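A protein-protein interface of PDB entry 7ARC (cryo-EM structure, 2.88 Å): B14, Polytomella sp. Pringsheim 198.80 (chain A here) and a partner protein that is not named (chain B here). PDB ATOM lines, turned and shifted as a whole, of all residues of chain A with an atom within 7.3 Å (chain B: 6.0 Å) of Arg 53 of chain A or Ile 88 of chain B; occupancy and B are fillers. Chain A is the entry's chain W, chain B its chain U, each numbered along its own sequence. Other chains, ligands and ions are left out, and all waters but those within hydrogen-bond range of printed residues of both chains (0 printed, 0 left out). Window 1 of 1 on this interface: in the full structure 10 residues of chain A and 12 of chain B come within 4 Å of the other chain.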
ATOM      1  N   TYR A  27      -5.565 -19.294 -15.447  1.00  0.00           N
ATOM      2  CA  TYR A  27      -6.344 -18.081 -15.221  1.00  0.00           C
ATOM      3  C   TYR A  27      -5.549 -16.840 -15.605  1.00  0.00           C
ATOM      4  O   TYR A  27      -6.105 -15.891 -16.168  1.00  0.00           O
ATOM      5  CB  TYR A  27      -6.793 -18.010 -13.762  1.00  0.00           C
ATOM      6  CG  TYR A  27      -7.671 -16.821 -13.457  1.00  0.00           C
ATOM      7  CD1 TYR A  27      -8.896 -16.659 -14.090  1.00  0.00           C
ATOM      8  CD2 TYR A  27      -7.280 -15.862 -12.535  1.00  0.00           C
ATOM      9  CE1 TYR A  27      -9.702 -15.575 -13.816  1.00  0.00           C
ATOM     10  CE2 TYR A  27      -8.082 -14.775 -12.254  1.00  0.00           C
ATOM     11  CZ  TYR A  27      -9.292 -14.638 -12.897  1.00  0.00           C
ATOM     12  OH  TYR A  27     -10.092 -13.555 -12.621  1.00  0.00           O
ATOM     13  N   LEU A  28      -4.251 -16.818 -15.293  1.00  0.00           N
ATOM     14  CA  LEU A  28      -3.418 -15.693 -15.702  1.00  0.00           C
ATOM     15  C   LEU A  28      -3.366 -15.572 -17.216  1.00  0.00           C
ATOM     16  O   LEU A  28      -3.430 -14.465 -17.762  1.00  0.00           O
ATOM     17  CB  LEU A  28      -1.999 -15.851 -15.159  1.00  0.00           C
ATOM     18  CG  LEU A  28      -1.640 -15.322 -13.779  1.00  0.00           C
ATOM     19  CD1 LEU A  28      -0.489 -16.116 -13.197  1.00  0.00           C
ATOM     20  CD2 LEU A  28      -1.269 -13.859 -13.900  1.00  0.00           C
ATOM     21  N   ALA A  30      -5.698 -16.538 -19.321  1.00  0.00           N
ATOM     22  CA  ALA A  30      -6.994 -16.032 -19.766  1.00  0.00           C
ATOM     23  C   ALA A  30      -7.117 -14.530 -19.531  1.00  0.00           C
ATOM     24  O   ALA A  30      -7.555 -13.782 -20.417  1.00  0.00           O
ATOM     25  CB  ALA A  30      -8.116 -16.784 -19.053  1.00  0.00           C
ATOM     26  N   CYS A  31      -6.727 -14.065 -18.341  1.00  0.00           N
ATOM     27  CA  CYS A  31      -6.812 -12.637 -18.044  1.00  0.00           C
ATOM     28  C   CYS A  31      -5.924 -11.822 -18.972  1.00  0.00           C
ATOM     29  O   CYS A  31      -6.329 -10.759 -19.453  1.00  0.00           O
ATOM     30  CB  CYS A  31      -6.448 -12.371 -16.584  1.00  0.00           C
ATOM     31  SG  CYS A  31      -7.473 -13.249 -15.392  1.00  0.00           S
ATOM     32  N   ARG A  32      -4.706 -12.299 -19.231  1.00  0.00           N
ATOM     33  CA  ARG A  32      -3.807 -11.562 -20.111  1.00  0.00           C
ATOM     34  C   ARG A  32      -4.296 -11.570 -21.554  1.00  0.00           C
ATOM     35  O   ARG A  32      -4.081 -10.594 -22.280  1.00  0.00           O
ATOM     36  CB  ARG A  32      -2.394 -12.134 -20.006  1.00  0.00           C
ATOM     37  CG  ARG A  32      -1.744 -11.859 -18.660  1.00  0.00           C
ATOM     38  CD  ARG A  32      -0.764 -10.704 -18.730  1.00  0.00           C
ATOM     39  NE  ARG A  32      -0.206 -10.386 -17.420  1.00  0.00           N
ATOM     40  CZ  ARG A  32       0.988 -10.773 -16.996  1.00  0.00           C
ATOM     41  NH1 ARG A  32       1.795 -11.489 -17.760  1.00  0.00           N
ATOM     42  NH2 ARG A  32       1.387 -10.426 -15.775  1.00  0.00           N
ATOM     43  N   LEU A  34      -7.460 -11.642 -22.436  1.00  0.00           N
ATOM     44  CA  LEU A  34      -8.786 -11.028 -22.544  1.00  0.00           C
ATOM     45  C   LEU A  34      -8.827  -9.794 -23.443  1.00  0.00           C
ATOM     46  O   LEU A  34      -9.742  -9.705 -24.281  1.00  0.00           O
ATOM     47  CB  LEU A  34      -9.307 -10.702 -21.141  1.00  0.00           C
ATOM     48  CG  LEU A  34     -10.299 -11.682 -20.522  1.00  0.00           C
ATOM     49  CD1 LEU A  34     -10.818 -11.135 -19.213  1.00  0.00           C
ATOM     50  CD2 LEU A  34     -11.446 -11.947 -21.471  1.00  0.00           C
ATOM     51  N   PRO A  35      -7.932  -8.804 -23.313  1.00  0.00           N
ATOM     52  CA  PRO A  35      -8.023  -7.646 -24.220  1.00  0.00           C
ATOM     53  C   PRO A  35      -7.906  -8.012 -25.690  1.00  0.00           C
ATOM     54  O   PRO A  35      -8.567  -7.393 -26.534  1.00  0.00           O
ATOM     55  CB  PRO A  35      -6.862  -6.749 -23.761  1.00  0.00           C
ATOM     56  CG  PRO A  35      -5.975  -7.632 -22.961  1.00  0.00           C
ATOM     57  CD  PRO A  35      -6.883  -8.605 -22.300  1.00  0.00           C
ATOM     58  N   HIS A  38     -11.244  -9.218 -26.767  1.00  0.00           N
ATOM     59  CA  HIS A  38     -12.127  -8.053 -26.813  1.00  0.00           C
ATOM     60  C   HIS A  38     -11.960  -7.269 -28.108  1.00  0.00           C
ATOM     61  O   HIS A  38     -12.948  -6.883 -28.745  1.00  0.00           O
ATOM     62  CB  HIS A  38     -11.883  -7.152 -25.606  1.00  0.00           C
ATOM     63  CG  HIS A  38     -12.738  -7.489 -24.428  1.00  0.00           C
ATOM     64  ND1 HIS A  38     -13.205  -6.534 -23.550  1.00  0.00           N
ATOM     65  CD2 HIS A  38     -13.215  -8.675 -23.984  1.00  0.00           C
ATOM     66  CE1 HIS A  38     -13.931  -7.119 -22.615  1.00  0.00           C
ATOM     67  NE2 HIS A  38     -13.953  -8.418 -22.854  1.00  0.00           N
ATOM     68  N   THR A  47     -19.108  -5.079 -23.337  1.00  0.00           N
ATOM     69  CA  THR A  47     -18.629  -5.556 -22.050  1.00  0.00           C
ATOM     70  C   THR A  47     -17.271  -4.946 -21.736  1.00  0.00           C
ATOM     71  O   THR A  47     -16.514  -4.554 -22.629  1.00  0.00           O
ATOM     72  CB  THR A  47     -18.545  -7.089 -22.016  1.00  0.00           C
ATOM     73  OG1 THR A  47     -18.285  -7.529 -20.677  1.00  0.00           O
ATOM     74  CG2 THR A  47     -17.446  -7.590 -22.936  1.00  0.00           C
ATOM     75  N   SER A  48     -16.981  -4.870 -20.443  1.00  0.00           N
ATOM     76  CA  SER A  48     -15.716  -4.391 -19.910  1.00  0.00           C
ATOM     77  C   SER A  48     -14.796  -5.558 -19.571  1.00  0.00           C
ATOM     78  O   SER A  48     -15.229  -6.705 -19.442  1.00  0.00           O
ATOM     79  CB  SER A  48     -15.949  -3.529 -18.666  1.00  0.00           C
ATOM     80  OG  SER A  48     -14.723  -3.081 -18.115  1.00  0.00           O
ATOM     81  N   LEU A  49     -13.505  -5.247 -19.435  1.00  0.00           N
ATOM     82  CA  LEU A  49     -12.524  -6.279 -19.113  1.00  0.00           C
ATOM     83  C   LEU A  49     -12.796  -6.854 -17.730  1.00  0.00           C
ATOM     84  O   LEU A  49     -12.733  -8.073 -17.528  1.00  0.00           O
ATOM     85  CB  LEU A  49     -11.108  -5.713 -19.202  1.00  0.00           C
ATOM     86  CG  LEU A  49     -10.560  -5.532 -20.619  1.00  0.00           C
ATOM     87  CD1 LEU A  49      -9.452  -4.492 -20.639  1.00  0.00           C
ATOM     88  CD2 LEU A  49     -10.074  -6.854 -21.183  1.00  0.00           C
ATOM     89  N   LYS A  50     -13.096  -5.980 -16.765  1.00  0.00           N
ATOM     90  CA  LYS A  50     -13.417  -6.419 -15.412  1.00  0.00           C
ATOM     91  C   LYS A  50     -14.646  -7.316 -15.411  1.00  0.00           C
ATOM     92  O   LYS A  50     -14.694  -8.322 -14.689  1.00  0.00           O
ATOM     93  CB  LYS A  50     -13.664  -5.186 -14.544  1.00  0.00           C
ATOM     94  CG  LYS A  50     -13.995  -5.425 -13.080  1.00  0.00           C
ATOM     95  CD  LYS A  50     -12.838  -5.945 -12.266  1.00  0.00           C
ATOM     96  CE  LYS A  50     -13.252  -6.033 -10.804  1.00  0.00           C
ATOM     97  NZ  LYS A  50     -12.190  -6.594  -9.934  1.00  0.00           N
ATOM     98  N   GLU A  51     -15.642  -6.976 -16.229  1.00  0.00           N
ATOM     99  CA  GLU A  51     -16.879  -7.746 -16.255  1.00  0.00           C
ATOM    100  C   GLU A  51     -16.630  -9.181 -16.708  1.00  0.00           C
ATOM    101  O   GLU A  51     -17.212 -10.122 -16.158  1.00  0.00           O
ATOM    102  CB  GLU A  51     -17.898  -7.049 -17.157  1.00  0.00           C
ATOM    103  CG  GLU A  51     -19.261  -7.711 -17.202  1.00  0.00           C
ATOM    104  CD  GLU A  51     -20.246  -6.946 -18.064  1.00  0.00           C
ATOM    105  OE1 GLU A  51     -19.855  -5.911 -18.643  1.00  0.00           O
ATOM    106  OE2 GLU A  51     -21.415  -7.378 -18.161  1.00  0.00           O
ATOM    107  N   MET A  52     -15.758  -9.371 -17.703  1.00  0.00           N
ATOM    108  CA  MET A  52     -15.420 -10.723 -18.143  1.00  0.00           C
ATOM    109  C   MET A  52     -14.520 -11.431 -17.138  1.00  0.00           C
ATOM    110  O   MET A  52     -14.644 -12.649 -16.931  1.00  0.00           O
ATOM    111  CB  MET A  52     -14.746 -10.670 -19.512  1.00  0.00           C
ATOM    112  CG  MET A  52     -15.640 -10.175 -20.629  1.00  0.00           C
ATOM    113  SD  MET A  52     -17.075 -11.235 -20.869  1.00  0.00           S
ATOM    114  CE  MET A  52     -16.292 -12.701 -21.532  1.00  0.00           C
ATOM    115  N   ARG A  53     -13.584 -10.693 -16.535  1.00  0.00           N
ATOM    116  CA  ARG A  53     -12.741 -11.266 -15.492  1.00  0.00           C
ATOM    117  C   ARG A  53     -13.571 -11.820 -14.344  1.00  0.00           C
ATOM    118  O   ARG A  53     -13.151 -12.775 -13.682  1.00  0.00           O
ATOM    119  CB  ARG A  53     -11.758 -10.215 -14.977  1.00  0.00           C
ATOM    120  CG  ARG A  53     -10.509 -10.074 -15.824  1.00  0.00           C
ATOM    121  CD  ARG A  53      -9.341  -9.538 -15.020  1.00  0.00           C
ATOM    122  NE  ARG A  53      -9.682  -8.310 -14.314  1.00  0.00           N
ATOM    123  CZ  ARG A  53      -9.422  -7.091 -14.764  1.00  0.00           C
ATOM    124  NH1 ARG A  53      -8.810  -6.897 -15.919  1.00  0.00           N
ATOM    125  NH2 ARG A  53      -9.783  -6.039 -14.035  1.00  0.00           N
ATOM    126  N   LEU A  54     -14.743 -11.234 -14.088  1.00  0.00           N
ATOM    127  CA  LEU A  54     -15.603 -11.782 -13.042  1.00  0.00           C
ATOM    128  C   LEU A  54     -16.224 -13.114 -13.458  1.00  0.00           C
ATOM    129  O   LEU A  54     -16.326 -14.035 -12.641  1.00  0.00           O
ATOM    130  CB  LEU A  54     -16.692 -10.778 -12.670  1.00  0.00           C
ATOM    131  CG  LEU A  54     -16.221  -9.375 -12.289  1.00  0.00           C
ATOM    132  CD1 LEU A  54     -17.374  -8.385 -12.313  1.00  0.00           C
ATOM    133  CD2 LEU A  54     -15.532  -9.381 -10.932  1.00  0.00           C
ATOM    134  N   ILE A  55     -16.649 -13.234 -14.719  1.00  0.00           N
ATOM    135  CA  ILE A  55     -17.268 -14.474 -15.182  1.00  0.00           C
ATOM    136  C   ILE A  55     -16.254 -15.611 -15.196  1.00  0.00           C
ATOM    137  O   ILE A  55     -16.587 -16.773 -14.899  1.00  0.00           O
ATOM    138  CB  ILE A  55     -17.897 -14.270 -16.572  1.00  0.00           C
ATOM    139  CG1 ILE A  55     -18.541 -12.889 -16.668  1.00  0.00           C
ATOM    140  CG2 ILE A  55     -18.920 -15.350 -16.856  1.00  0.00           C
ATOM    141  CD1 ILE A  55     -19.176 -12.608 -18.008  1.00  0.00           C
ATOM    142  N   ILE A  56     -15.013 -15.302 -15.577  1.00  0.00           N
ATOM    143  CA  ILE A  56     -14.005 -16.347 -15.724  1.00  0.00           C
ATOM    144  C   ILE A  56     -13.758 -17.051 -14.397  1.00  0.00           C
ATOM    145  O   ILE A  56     -13.518 -18.268 -14.359  1.00  0.00           O
ATOM    146  CB  ILE A  56     -12.707 -15.759 -16.302  1.00  0.00           C
ATOM    147  CG1 ILE A  56     -12.981 -15.160 -17.674  1.00  0.00           C
ATOM    148  CG2 ILE A  56     -11.653 -16.839 -16.447  1.00  0.00           C
ATOM    149  CD1 ILE A  56     -13.473 -16.156 -18.655  1.00  0.00           C
ATOM    150  N   LYS A  57     -13.834 -16.313 -13.286  1.00  0.00           N
ATOM    151  CA  LYS A  57     -13.622 -16.945 -11.990  1.00  0.00           C
ATOM    152  C   LYS A  57     -14.700 -17.976 -11.697  1.00  0.00           C
ATOM    153  O   LYS A  57     -14.400 -19.059 -11.192  1.00  0.00           O
ATOM    154  CB  LYS A  57     -13.592 -15.886 -10.891  1.00  0.00           C
ATOM    155  CG  LYS A  57     -12.430 -14.924 -10.983  1.00  0.00           C
ATOM    156  CD  LYS A  57     -12.400 -13.988  -9.789  1.00  0.00           C
ATOM    157  CE  LYS A  57     -13.528 -12.973  -9.863  1.00  0.00           C
ATOM    158  NZ  LYS A  57     -13.454 -11.978  -8.760  1.00  0.00           N
ATOM    159  N   ASP A  58     -15.962 -17.655 -11.989  1.00  0.00           N
ATOM    160  CA  ASP A  58     -17.042 -18.612 -11.756  1.00  0.00           C
ATOM    161  C   ASP A  58     -16.881 -19.846 -12.635  1.00  0.00           C
ATOM    162  O   ASP A  58     -17.108 -20.985 -12.188  1.00  0.00           O
ATOM    163  CB  ASP A  58     -18.393 -17.942 -11.990  1.00  0.00           C
ATOM    164  CG  ASP A  58     -18.712 -16.896 -10.937  1.00  0.00           C
ATOM    165  OD1 ASP A  58     -18.237 -17.043  -9.791  1.00  0.00           O
ATOM    166  OD2 ASP A  58     -19.435 -15.928 -11.252  1.00  0.00           O
ATOM    167  N   LYS B  83      -6.853 -13.164  -6.089  1.00  0.00           N
ATOM    168  CA  LYS B  83      -5.578 -12.453  -6.010  1.00  0.00           C
ATOM    169  C   LYS B  83      -5.058 -12.094  -7.396  1.00  0.00           C
ATOM    170  O   LYS B  83      -4.597 -10.969  -7.632  1.00  0.00           O
ATOM    171  CB  LYS B  83      -4.560 -13.321  -5.272  1.00  0.00           C
ATOM    172  CG  LYS B  83      -3.216 -12.670  -5.028  1.00  0.00           C
ATOM    173  CD  LYS B  83      -2.319 -13.591  -4.220  1.00  0.00           C
ATOM    174  CE  LYS B  83      -0.960 -12.967  -3.969  1.00  0.00           C
ATOM    175  NZ  LYS B  83      -0.078 -13.871  -3.180  1.00  0.00           N
ATOM    176  N   VAL B  84      -5.133 -13.037  -8.331  1.00  0.00           N
ATOM    177  CA  VAL B  84      -4.648 -12.770  -9.679  1.00  0.00           C
ATOM    178  C   VAL B  84      -5.491 -11.695 -10.354  1.00  0.00           C
ATOM    179  O   VAL B  84      -4.961 -10.792 -11.013  1.00  0.00           O
ATOM    180  CB  VAL B  84      -4.635 -14.070 -10.499  1.00  0.00           C
ATOM    181  CG1 VAL B  84      -4.241 -13.778 -11.925  1.00  0.00           C
ATOM    182  CG2 VAL B  84      -3.678 -15.064  -9.882  1.00  0.00           C
ATOM    183  N   GLU B  85      -6.812 -11.766 -10.191  1.00  0.00           N
ATOM    184  CA  GLU B  85      -7.678 -10.743 -10.763  1.00  0.00           C
ATOM    185  C   GLU B  85      -7.417  -9.365 -10.156  1.00  0.00           C
ATOM    186  O   GLU B  85      -7.453  -8.356 -10.868  1.00  0.00           O
ATOM    187  CB  GLU B  85      -9.139 -11.164 -10.591  1.00  0.00           C
ATOM    188  CG  GLU B  85     -10.142 -10.271 -11.282  1.00  0.00           C
ATOM    189  CD  GLU B  85     -10.501  -9.062 -10.462  1.00  0.00           C
ATOM    190  OE1 GLU B  85     -10.441  -9.144  -9.218  1.00  0.00           O
ATOM    191  OE2 GLU B  85     -10.819  -8.018 -11.064  1.00  0.00           O
ATOM    192  N   LEU B  86      -7.187  -9.288  -8.840  1.00  0.00           N
ATOM    193  CA  LEU B  86      -6.860  -7.993  -8.240  1.00  0.00           C
ATOM    194  C   LEU B  86      -5.556  -7.448  -8.811  1.00  0.00           C
ATOM    195  O   LEU B  86      -5.432  -6.244  -9.061  1.00  0.00           O
ATOM    196  CB  LEU B  86      -6.803  -8.061  -6.711  1.00  0.00           C
ATOM    197  CG  LEU B  86      -5.851  -8.908  -5.872  1.00  0.00           C
ATOM    198  CD1 LEU B  86      -4.496  -8.235  -5.720  1.00  0.00           C
ATOM    199  CD2 LEU B  86      -6.459  -9.171  -4.514  1.00  0.00           C
ATOM    200  N   LEU B  87      -4.561  -8.321  -8.996  1.00  0.00           N
ATOM    201  CA  LEU B  87      -3.317  -7.886  -9.622  1.00  0.00           C
ATOM    202  C   LEU B  87      -3.555  -7.378 -11.039  1.00  0.00           C
ATOM    203  O   LEU B  87      -2.923  -6.409 -11.468  1.00  0.00           O
ATOM    204  CB  LEU B  87      -2.296  -9.021  -9.615  1.00  0.00           C
ATOM    205  CG  LEU B  87      -1.820  -9.429  -8.220  1.00  0.00           C
ATOM    206  CD1 LEU B  87      -0.920 -10.645  -8.289  1.00  0.00           C
ATOM    207  CD2 LEU B  87      -1.107  -8.271  -7.548  1.00  0.00           C
ATOM    208  N   ILE B  88      -4.462  -8.011 -11.783  1.00  0.00           N
ATOM    209  CA  ILE B  88      -4.768  -7.530 -13.132  1.00  0.00           C
ATOM    210  C   ILE B  88      -5.483  -6.182 -13.068  1.00  0.00           C
ATOM    211  O   ILE B  88      -5.305  -5.313 -13.934  1.00  0.00           O
ATOM    212  CB  ILE B  88      -5.578  -8.577 -13.917  1.00  0.00           C
ATOM    213  CG1 ILE B  88      -4.843  -9.918 -13.932  1.00  0.00           C
ATOM    214  CG2 ILE B  88      -5.824  -8.107 -15.341  1.00  0.00           C
ATOM    215  CD1 ILE B  88      -3.716  -9.989 -14.936  1.00  0.00           C
ATOM    216  N   SER B  89      -6.322  -5.987 -12.054  1.00  0.00           N
ATOM    217  CA  SER B  89      -6.952  -4.684 -11.883  1.00  0.00           C
ATOM    218  C   SER B  89      -5.914  -3.607 -11.586  1.00  0.00           C
ATOM    219  O   SER B  89      -5.997  -2.496 -12.117  1.00  0.00           O
ATOM    220  CB  SER B  89      -7.992  -4.748 -10.766  1.00  0.00           C
ATOM    221  OG  SER B  89      -9.051  -5.627 -11.102  1.00  0.00           O
ATOM    222  N   LEU B  90      -4.923  -3.919 -10.745  1.00  0.00           N
ATOM    223  CA  LEU B  90      -3.793  -3.006 -10.564  1.00  0.00           C
ATOM    224  C   LEU B  90      -2.996  -2.817 -11.851  1.00  0.00           C
ATOM    225  O   LEU B  90      -2.417  -1.747 -12.070  1.00  0.00           O
ATOM    226  CB  LEU B  90      -2.886  -3.503  -9.438  1.00  0.00           C
ATOM    227  CG  LEU B  90      -3.610  -3.818  -8.129  1.00  0.00           C
ATOM    228  CD1 LEU B  90      -2.657  -4.416  -7.105  1.00  0.00           C
ATOM    229  CD2 LEU B  90      -4.279  -2.568  -7.584  1.00  0.00           C
ATOM    230  N   GLU B  91      -2.942  -3.846 -12.700  1.00  0.00           N
ATOM    231  CA  GLU B  91      -2.385  -3.695 -14.042  1.00  0.00           C
ATOM    232  C   GLU B  91      -3.099  -2.584 -14.791  1.00  0.00           C
ATOM    233  O   GLU B  91      -2.471  -1.746 -15.446  1.00  0.00           O
ATOM    234  CB  GLU B  91      -2.501  -5.013 -14.811  1.00  0.00           C
ATOM    235  CG  GLU B  91      -1.650  -6.141 -14.288  1.00  0.00           C
ATOM    236  CD  GLU B  91      -0.198  -5.864 -14.508  1.00  0.00           C
ATOM    237  OE1 GLU B  91       0.093  -5.207 -15.525  1.00  0.00           O
ATOM    238  OE2 GLU B  91       0.640  -6.273 -13.680  1.00  0.00           O
ATOM    239  N   GLU B  92      -4.429  -2.580 -14.722  1.00  0.00           N
ATOM    240  CA  GLU B  92      -5.184  -1.524 -15.390  1.00  0.00           C
ATOM    241  C   GLU B  92      -4.944  -0.171 -14.723  1.00  0.00           C
ATOM    242  O   GLU B  92      -4.753   0.839 -15.410  1.00  0.00           O
ATOM    243  CB  GLU B  92      -6.675  -1.862 -15.384  1.00  0.00           C
ATOM    244  CG  GLU B  92      -7.053  -3.080 -16.211  1.00  0.00           C
ATOM    245  CD  GLU B  92      -6.832  -2.874 -17.694  1.00  0.00           C
ATOM    246  OE1 GLU B  92      -6.975  -1.726 -18.165  1.00  0.00           O
ATOM    247  OE2 GLU B  92      -6.514  -3.860 -18.392  1.00  0.00           O
ATOM    248  N   ASP B  93      -4.952  -0.134 -13.389  1.00  0.00           N
ATOM    249  CA  ASP B  93      -4.753   1.118 -12.662  1.00  0.00           C
ATOM    250  C   ASP B  93      -3.369   1.707 -12.917  1.00  0.00           C
ATOM    251  O   ASP B  93      -3.235   2.790 -13.498  1.00  0.00           O
ATOM    252  CB  ASP B  93      -4.982   0.906 -11.163  1.00  0.00           C
ATOM    253  CG  ASP B  93      -6.446   0.706 -10.817  1.00  0.00           C
ATOM    254  OD1 ASP B  93      -7.185   1.711 -10.770  1.00  0.00           O
ATOM    255  OD2 ASP B  93      -6.858  -0.447 -10.575  1.00  0.00           O
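Arg 53 of chain A touches just these residues of chain B: Glu 85, Ile 88 and Ser 89. Of chain A, only Cys 31 and Arg 53 come within 4 Å of Ile 88 of chain B. Printed residues of chain A within 4 Å of Val 84 of chain B: Tyr 27 and Leu 28. Of the printed residues of chain A, Glu 85 of chain B touches Tyr 27 (3.3 Å), Lys 50 (2.3 Å) and Arg 53 (3.5 Å). Printed residues of chain B within 4 Å of Cys 31 of chain A: Ile 88. Of the printed residues of chain B, Tyr 27 of chain A touches Val 84 (3.7 Å) and Glu 85 (3.3 Å). Of the printed residues of chain B, Leu 28 of chain A touches Val 84. Ile 56 of chain A touches none of the printed residues of chain B. The nearest residue of chain A that does not touch Ile 88 of chain B is Arg 32 of chain A (4.3 Å).
Among the printed residues, merely in contact across the chains: Arg 53 of chain A with Ile 88 of chain B, Tyr 27 of chain A with Glu 85 of chain B, Leu 28 of chain A with Val 84 of chain B, Tyr 27 of chain A with Val 84 of chain B, Leu 49 of chain A with Glu 92 of chain B and Cys 31 of chain A with Ile 88 of chain B.
OE2 of Glu 85 of chain B is in hydrogen-bond range of OG of Ser 89 of chain B. O of Ser 89 of chain B lies close to OD2 of Asp 93 of chain B (2.7 Å). SG of Cys 31 of chain A is in hydrogen-bond range of O of Tyr 27 of chain A, at 3.1 Å. O of Arg 53 of chain A sits at hydrogen-bond distance from OH of Tyr 27 of chain A, at 3.3 Å.
Hydrophobic or aromatic side chains of chain A that line the printed part of chain B: Tyr 27, Leu 28 and Leu 49.
OE1 of Glu 85 of chain B is in salt-bridge range of NZ of Lys 50 of chain A, at 3.2 Å. OE2 of Glu 85 of chain B is in salt-bridge range of NE of Arg 53 of chain A, at 3.5 Å. NZ of Lys 50 of chain A is in hydrogen-bond range of OG of Ser 89 of chain B. The side-chain hydroxyl of Ser 89 of chain B is in hydrogen-bond range of the guanidinium group of Arg 53 of chain A, 3.1 Å away.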
